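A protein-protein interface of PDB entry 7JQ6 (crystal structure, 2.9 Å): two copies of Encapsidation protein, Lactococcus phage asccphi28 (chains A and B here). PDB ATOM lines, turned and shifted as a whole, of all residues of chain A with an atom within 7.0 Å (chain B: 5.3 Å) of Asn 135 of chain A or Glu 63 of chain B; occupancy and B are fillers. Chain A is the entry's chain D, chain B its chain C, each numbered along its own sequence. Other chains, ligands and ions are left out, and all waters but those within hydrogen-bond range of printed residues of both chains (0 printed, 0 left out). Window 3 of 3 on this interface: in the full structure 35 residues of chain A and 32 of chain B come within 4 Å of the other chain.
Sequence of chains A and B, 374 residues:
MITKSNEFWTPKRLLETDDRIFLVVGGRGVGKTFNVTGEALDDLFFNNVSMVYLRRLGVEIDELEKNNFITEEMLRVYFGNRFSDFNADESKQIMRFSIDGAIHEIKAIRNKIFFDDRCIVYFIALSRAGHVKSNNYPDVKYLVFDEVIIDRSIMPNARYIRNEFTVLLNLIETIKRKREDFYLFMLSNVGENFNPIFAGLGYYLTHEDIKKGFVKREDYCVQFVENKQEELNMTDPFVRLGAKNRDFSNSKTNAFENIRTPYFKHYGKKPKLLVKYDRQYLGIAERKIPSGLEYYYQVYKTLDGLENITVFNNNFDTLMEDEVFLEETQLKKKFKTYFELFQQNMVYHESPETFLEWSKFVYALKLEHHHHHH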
ATOM      1  N   ILE A 124     -36.086 -22.140  -0.089  1.00  0.00           N
ATOM      2  CA  ILE A 124     -35.510 -22.625  -1.335  1.00  0.00           C
ATOM      3  C   ILE A 124     -36.252 -23.885  -1.755  1.00  0.00           C
ATOM      4  O   ILE A 124     -36.755 -24.644  -0.920  1.00  0.00           O
ATOM      5  CB  ILE A 124     -33.990 -22.892  -1.219  1.00  0.00           C
ATOM      6  CG1 ILE A 124     -33.681 -23.904  -0.113  1.00  0.00           C
ATOM      7  CG2 ILE A 124     -33.235 -21.590  -0.964  1.00  0.00           C
ATOM      8  CD1 ILE A 124     -33.902 -25.354  -0.512  1.00  0.00           C
ATOM      9  N   ALA A 125     -36.334 -24.091  -3.066  1.00  0.00           N
ATOM     10  CA  ALA A 125     -37.070 -25.198  -3.657  1.00  0.00           C
ATOM     11  C   ALA A 125     -36.099 -26.180  -4.292  1.00  0.00           C
ATOM     12  O   ALA A 125     -35.121 -25.775  -4.928  1.00  0.00           O
ATOM     13  CB  ALA A 125     -38.058 -24.700  -4.710  1.00  0.00           C
ATOM     14  N   SER A 127     -36.400 -28.082  -6.860  1.00  0.00           N
ATOM     15  CA  SER A 127     -36.329 -27.979  -8.315  1.00  0.00           C
ATOM     16  C   SER A 127     -35.355 -26.891  -8.752  1.00  0.00           C
ATOM     17  O   SER A 127     -34.660 -27.043  -9.764  1.00  0.00           O
ATOM     18  CB  SER A 127     -37.718 -27.717  -8.897  1.00  0.00           C
ATOM     19  OG  SER A 127     -38.245 -26.486  -8.439  1.00  0.00           O
ATOM     20  N   ARG A 128     -35.284 -25.789  -8.004  1.00  0.00           N
ATOM     21  CA  ARG A 128     -34.368 -24.714  -8.365  1.00  0.00           C
ATOM     22  C   ARG A 128     -33.023 -24.835  -7.657  1.00  0.00           C
ATOM     23  O   ARG A 128     -31.982 -24.551  -8.260  1.00  0.00           O
ATOM     24  CB  ARG A 128     -34.989 -23.350  -8.046  1.00  0.00           C
ATOM     25  CG  ARG A 128     -36.421 -23.172  -8.531  1.00  0.00           C
ATOM     26  CD  ARG A 128     -36.983 -21.829  -8.084  1.00  0.00           C
ATOM     27  NE  ARG A 128     -38.429 -21.735  -8.264  1.00  0.00           N
ATOM     28  CZ  ARG A 128     -39.180 -20.745  -7.790  1.00  0.00           C
ATOM     29  NH1 ARG A 128     -38.623 -19.753  -7.105  1.00  0.00           N
ATOM     30  NH2 ARG A 128     -40.490 -20.745  -7.996  1.00  0.00           N
ATOM     31  N   ALA A 129     -33.017 -25.258  -6.390  1.00  0.00           N
ATOM     32  CA  ALA A 129     -31.768 -25.297  -5.636  1.00  0.00           C
ATOM     33  C   ALA A 129     -30.768 -26.254  -6.272  1.00  0.00           C
ATOM     34  O   ALA A 129     -29.558 -26.002  -6.257  1.00  0.00           O
ATOM     35  CB  ALA A 129     -32.042 -25.700  -4.187  1.00  0.00           C
ATOM     36  N   GLY A 130     -31.256 -27.356  -6.843  1.00  0.00           N
ATOM     37  CA  GLY A 130     -30.360 -28.324  -7.449  1.00  0.00           C
ATOM     38  C   GLY A 130     -29.572 -27.759  -8.612  1.00  0.00           C
ATOM     39  O   GLY A 130     -28.439 -28.178  -8.860  1.00  0.00           O
ATOM     40  N   HIS A 131     -30.153 -26.799  -9.336  1.00  0.00           N
ATOM     41  CA  HIS A 131     -29.524 -26.292 -10.550  1.00  0.00           C
ATOM     42  C   HIS A 131     -28.262 -25.484 -10.269  1.00  0.00           C
ATOM     43  O   HIS A 131     -27.410 -25.373 -11.155  1.00  0.00           O
ATOM     44  CB  HIS A 131     -30.522 -25.441 -11.339  1.00  0.00           C
ATOM     45  CG  HIS A 131     -31.512 -26.245 -12.127  1.00  0.00           C
ATOM     46  ND1 HIS A 131     -32.440 -27.075 -11.535  1.00  0.00           N
ATOM     47  CD2 HIS A 131     -31.718 -26.344 -13.462  1.00  0.00           C
ATOM     48  CE1 HIS A 131     -33.175 -27.650 -12.471  1.00  0.00           C
ATOM     49  NE2 HIS A 131     -32.757 -27.224 -13.649  1.00  0.00           N
ATOM     50  N   VAL A 132     -28.118 -24.921  -9.071  1.00  0.00           N
ATOM     51  CA  VAL A 132     -26.928 -24.164  -8.703  1.00  0.00           C
ATOM     52  C   VAL A 132     -26.467 -24.624  -7.328  1.00  0.00           C
ATOM     53  O   VAL A 132     -27.255 -24.636  -6.375  1.00  0.00           O
ATOM     54  CB  VAL A 132     -27.184 -22.644  -8.706  1.00  0.00           C
ATOM     55  CG1 VAL A 132     -27.680 -22.196 -10.068  1.00  0.00           C
ATOM     56  CG2 VAL A 132     -28.173 -22.255  -7.617  1.00  0.00           C
ATOM     57  N   LYS A 133     -25.194 -25.010  -7.229  1.00  0.00           N
ATOM     58  CA  LYS A 133     -24.593 -25.391  -5.961  1.00  0.00           C
ATOM     59  C   LYS A 133     -23.454 -24.467  -5.551  1.00  0.00           C
ATOM     60  O   LYS A 133     -22.821 -24.711  -4.518  1.00  0.00           O
ATOM     61  CB  LYS A 133     -24.084 -26.836  -6.020  1.00  0.00           C
ATOM     62  CG  LYS A 133     -25.189 -27.875  -6.153  1.00  0.00           C
ATOM     63  CD  LYS A 133     -26.138 -27.843  -4.960  1.00  0.00           C
ATOM     64  CE  LYS A 133     -27.245 -28.869  -5.105  1.00  0.00           C
ATOM     65  NZ  LYS A 133     -26.711 -30.252  -5.123  1.00  0.00           N
ATOM     66  N   SER A 134     -23.171 -23.422  -6.330  1.00  0.00           N
ATOM     67  CA  SER A 134     -22.229 -22.404  -5.888  1.00  0.00           C
ATOM     68  C   SER A 134     -22.774 -21.613  -4.707  1.00  0.00           C
ATOM     69  O   SER A 134     -21.987 -21.024  -3.957  1.00  0.00           O
ATOM     70  CB  SER A 134     -21.899 -21.458  -7.041  1.00  0.00           C
ATOM     71  OG  SER A 134     -21.449 -22.181  -8.175  1.00  0.00           O
ATOM     72  N   ASN A 135     -24.094 -21.583  -4.533  1.00  0.00           N
ATOM     73  CA  ASN A 135     -24.688 -20.959  -3.359  1.00  0.00           C
ATOM     74  C   ASN A 135     -24.106 -21.567  -2.090  1.00  0.00           C
ATOM     75  O   ASN A 135     -23.731 -22.741  -2.053  1.00  0.00           O
ATOM     76  CB  ASN A 135     -26.208 -21.136  -3.368  1.00  0.00           C
ATOM     77  CG  ASN A 135     -26.913 -20.071  -4.177  1.00  0.00           C
ATOM     78  OD1 ASN A 135     -26.537 -18.903  -4.140  1.00  0.00           O
ATOM     79  ND2 ASN A 135     -27.944 -20.469  -4.913  1.00  0.00           N
ATOM     80  N   ASN A 136     -24.035 -20.753  -1.040  1.00  0.00           N
ATOM     81  CA  ASN A 136     -23.521 -21.215   0.242  1.00  0.00           C
ATOM     82  C   ASN A 136     -24.265 -20.496   1.356  1.00  0.00           C
ATOM     83  O   ASN A 136     -24.379 -19.267   1.343  1.00  0.00           O
ATOM     84  CB  ASN A 136     -22.011 -20.974   0.349  1.00  0.00           C
ATOM     85  CG  ASN A 136     -21.290 -22.096   1.076  1.00  0.00           C
ATOM     86  OD1 ASN A 136     -21.865 -23.153   1.343  1.00  0.00           O
ATOM     87  ND2 ASN A 136     -20.021 -21.875   1.391  1.00  0.00           N
ATOM     88  N   TYR A 137     -24.775 -21.272   2.305  1.00  0.00           N
ATOM     89  CA  TYR A 137     -25.524 -20.760   3.448  1.00  0.00           C
ATOM     90  C   TYR A 137     -24.664 -20.868   4.698  1.00  0.00           C
ATOM     91  O   TYR A 137     -24.470 -21.979   5.215  1.00  0.00           O
ATOM     92  CB  TYR A 137     -26.839 -21.519   3.615  1.00  0.00           C
ATOM     93  CG  TYR A 137     -27.636 -21.580   2.329  1.00  0.00           C
ATOM     94  CD1 TYR A 137     -27.563 -20.548   1.401  1.00  0.00           C
ATOM     95  CD2 TYR A 137     -28.460 -22.658   2.041  1.00  0.00           C
ATOM     96  CE1 TYR A 137     -28.282 -20.587   0.226  1.00  0.00           C
ATOM     97  CE2 TYR A 137     -29.186 -22.705   0.861  1.00  0.00           C
ATOM     98  CZ  TYR A 137     -29.092 -21.665  -0.041  1.00  0.00           C
ATOM     99  OH  TYR A 137     -29.805 -21.693  -1.215  1.00  0.00           O
ATOM    100  N   THR A 174     -24.037 -28.821   0.414  1.00  0.00           N
ATOM    101  CA  THR A 174     -23.881 -27.388   0.184  1.00  0.00           C
ATOM    102  C   THR A 174     -24.400 -26.598   1.379  1.00  0.00           C
ATOM    103  O   THR A 174     -23.745 -25.661   1.853  1.00  0.00           O
ATOM    104  CB  THR A 174     -24.604 -26.974  -1.097  1.00  0.00           C
ATOM    105  OG1 THR A 174     -23.988 -27.612  -2.222  1.00  0.00           O
ATOM    106  CG2 THR A 174     -24.542 -25.463  -1.283  1.00  0.00           C
ATOM    107  N   ILE A 175     -25.579 -26.966   1.884  1.00  0.00           N
ATOM    108  CA  ILE A 175     -26.141 -26.286   3.045  1.00  0.00           C
ATOM    109  C   ILE A 175     -25.275 -26.548   4.269  1.00  0.00           C
ATOM    110  O   ILE A 175     -24.938 -25.628   5.024  1.00  0.00           O
ATOM    111  CB  ILE A 175     -27.596 -26.741   3.275  1.00  0.00           C
ATOM    112  CG1 ILE A 175     -28.479 -26.286   2.109  1.00  0.00           C
ATOM    113  CG2 ILE A 175     -28.124 -26.201   4.604  1.00  0.00           C
ATOM    114  CD1 ILE A 175     -29.955 -26.605   2.273  1.00  0.00           C
ATOM    115  N   VAL B  59     -30.749 -18.449 -15.591  1.00  0.00           N
ATOM    116  CA  VAL B  59     -31.422 -19.094 -14.468  1.00  0.00           C
ATOM    117  C   VAL B  59     -30.436 -19.333 -13.334  1.00  0.00           C
ATOM    118  O   VAL B  59     -30.784 -19.223 -12.151  1.00  0.00           O
ATOM    119  CB  VAL B  59     -32.081 -20.410 -14.926  1.00  0.00           C
ATOM    120  CG1 VAL B  59     -32.760 -21.101 -13.751  1.00  0.00           C
ATOM    121  CG2 VAL B  59     -33.067 -20.155 -16.064  1.00  0.00           C
ATOM    122  N   GLU B  60     -29.187 -19.664 -13.676  1.00  0.00           N
ATOM    123  CA  GLU B  60     -28.191 -19.985 -12.660  1.00  0.00           C
ATOM    124  C   GLU B  60     -27.842 -18.772 -11.807  1.00  0.00           C
ATOM    125  O   GLU B  60     -27.494 -18.925 -10.631  1.00  0.00           O
ATOM    126  CB  GLU B  60     -26.928 -20.542 -13.326  1.00  0.00           C
ATOM    127  CG  GLU B  60     -27.199 -21.589 -14.407  1.00  0.00           C
ATOM    128  CD  GLU B  60     -25.943 -22.308 -14.886  1.00  0.00           C
ATOM    129  OE1 GLU B  60     -25.048 -22.580 -14.060  1.00  0.00           O
ATOM    130  OE2 GLU B  60     -25.848 -22.604 -16.096  1.00  0.00           O
ATOM    131  N   ILE B  61     -27.921 -17.568 -12.375  1.00  0.00           N
ATOM    132  CA  ILE B  61     -27.535 -16.366 -11.646  1.00  0.00           C
ATOM    133  C   ILE B  61     -28.649 -15.887 -10.726  1.00  0.00           C
ATOM    134  O   ILE B  61     -28.396 -15.498  -9.580  1.00  0.00           O
ATOM    135  CB  ILE B  61     -27.114 -15.275 -12.644  1.00  0.00           C
ATOM    136  CG1 ILE B  61     -25.790 -15.682 -13.289  1.00  0.00           C
ATOM    137  CG2 ILE B  61     -27.022 -13.920 -11.960  1.00  0.00           C
ATOM    138  CD1 ILE B  61     -25.305 -14.739 -14.339  1.00  0.00           C
ATOM    139  N   ASP B  62     -29.895 -15.900 -11.199  1.00  0.00           N
ATOM    140  CA  ASP B  62     -30.996 -15.417 -10.373  1.00  0.00           C
ATOM    141  C   ASP B  62     -31.098 -16.215  -9.082  1.00  0.00           C
ATOM    142  O   ASP B  62     -31.345 -15.651  -8.010  1.00  0.00           O
ATOM    143  CB  ASP B  62     -32.302 -15.485 -11.162  1.00  0.00           C
ATOM    144  CG  ASP B  62     -32.249 -14.670 -12.441  1.00  0.00           C
ATOM    145  OD1 ASP B  62     -31.406 -13.751 -12.524  1.00  0.00           O
ATOM    146  OD2 ASP B  62     -33.043 -14.950 -13.364  1.00  0.00           O
ATOM    147  N   GLU B  63     -30.906 -17.533  -9.163  1.00  0.00           N
ATOM    148  CA  GLU B  63     -30.942 -18.377  -7.978  1.00  0.00           C
ATOM    149  C   GLU B  63     -29.728 -18.168  -7.083  1.00  0.00           C
ATOM    150  O   GLU B  63     -29.792 -18.477  -5.889  1.00  0.00           O
ATOM    151  CB  GLU B  63     -31.027 -19.846  -8.400  1.00  0.00           C
ATOM    152  CG  GLU B  63     -32.212 -20.157  -9.306  1.00  0.00           C
ATOM    153  CD  GLU B  63     -32.281 -21.620  -9.698  1.00  0.00           C
ATOM    154  OE1 GLU B  63     -31.318 -22.360  -9.405  1.00  0.00           O
ATOM    155  OE2 GLU B  63     -33.297 -22.029 -10.302  1.00  0.00           O
ATOM    156  N   LEU B  64     -28.630 -17.652  -7.627  1.00  0.00           N
ATOM    157  CA  LEU B  64     -27.408 -17.482  -6.853  1.00  0.00           C
ATOM    158  C   LEU B  64     -27.595 -16.426  -5.770  1.00  0.00           C
ATOM    159  O   LEU B  64     -28.210 -15.380  -5.994  1.00  0.00           O
ATOM    160  CB  LEU B  64     -26.256 -17.099  -7.781  1.00  0.00           C
ATOM    161  CG  LEU B  64     -24.977 -16.542  -7.159  1.00  0.00           C
ATOM    162  CD1 LEU B  64     -24.292 -17.585  -6.295  1.00  0.00           C
ATOM    163  CD2 LEU B  64     -24.046 -16.063  -8.258  1.00  0.00           C
ATOM    164  N   GLU B  65     -27.043 -16.708  -4.590  1.00  0.00           N
ATOM    165  CA  GLU B  65     -27.137 -15.825  -3.427  1.00  0.00           C
ATOM    166  C   GLU B  65     -26.068 -14.747  -3.507  1.00  0.00           C
ATOM    167  O   GLU B  65     -24.890 -15.001  -3.249  1.00  0.00           O
ATOM    168  CB  GLU B  65     -27.003 -16.623  -2.136  1.00  0.00           C
ATOM    169  CG  GLU B  65     -28.212 -17.470  -1.807  1.00  0.00           C
ATOM    170  CD  GLU B  65     -29.292 -16.681  -1.085  1.00  0.00           C
ATOM    171  OE1 GLU B  65     -29.073 -15.477  -0.820  1.00  0.00           O
ATOM    172  OE2 GLU B  65     -30.355 -17.264  -0.780  1.00  0.00           O
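OE1 of Glu 63 of chain B lies close to O of Arg 128 of chain A (2.6 Å). O of Glu 63 of chain B lies within hydrogen-bond range of ND2 of Asn 135 of chain A (2.9 Å). The side-chain amide oxygen (OD1) of Asn 135 of chain A lies close to the backbone NH (N) of Glu 65 of chain B (2.3 Å).
O of Ser 127 of chain A lies within hydrogen-bond range of ND1 of His 131 of chain A (2.8 Å).
CB of His 131 of chain A touches OE1 of Glu 63 of chain B (3.7 Å). CG1 of Val 132 of chain A touches O of Glu 60 of chain B, at 3.3 Å. Val 132 of chain A touches Glu 63 of chain B (CG2 to OE1, 3.6 Å). OD1 of Asn 135 of chain A touches C of Leu 64 of chain B, at 3.1 Å. Tyr 137 of chain A touches Glu 65 of chain B.
Asn 135 of chain A touches just these residues of chain B: Glu 63 (2.9 Å), Leu 64 (3.1 Å) and Glu 65 (2.3 Å). Printed residues of chain A within 4 Å of Glu 63 of chain B: Arg 128, His 131, Val 132 and Asn 135. Printed residues of chain B within 4 Å of Tyr 137 of chain A: Glu 65. Of the printed residues of chain A, Leu 64 of chain B touches Asn 135 (3.1 Å). Of the printed residues of chain B, Arg 128 of chain A touches Glu 63. Of the printed residues of chain B, His 131 of chain A touches Glu 63 (3.7 Å). Printed residues of chain A within 4 Å of Glu 65 of chain B: Asn 135 (2.3 Å) and Tyr 137 (3.7 Å). The nearest residue of chain A that does not touch Glu 63 of chain B is Ala 129 of chain A (4.5 Å).
Of the 15 printed residues of chain A, 5 touch a printed residue of chain B. Printed residues of chain A that touch a printed residue of chain B: Arg 128, His 131, Val 132, Asn 135 and Tyr 137. Of the 7 printed residues of chain B, 4 touch a printed residue of chain A. Printed residues of chain B that touch a printed residue of chain A: Glu 60, Glu 63, Leu 64 and Glu 65. Among the printed residues, 8 pairs touch across the chains. Among the printed residues, no Asp or Glu carboxylate lies within 4 Å of a Lys or Arg side-chain nitrogen of the other chain.
No position is printed for both chains.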
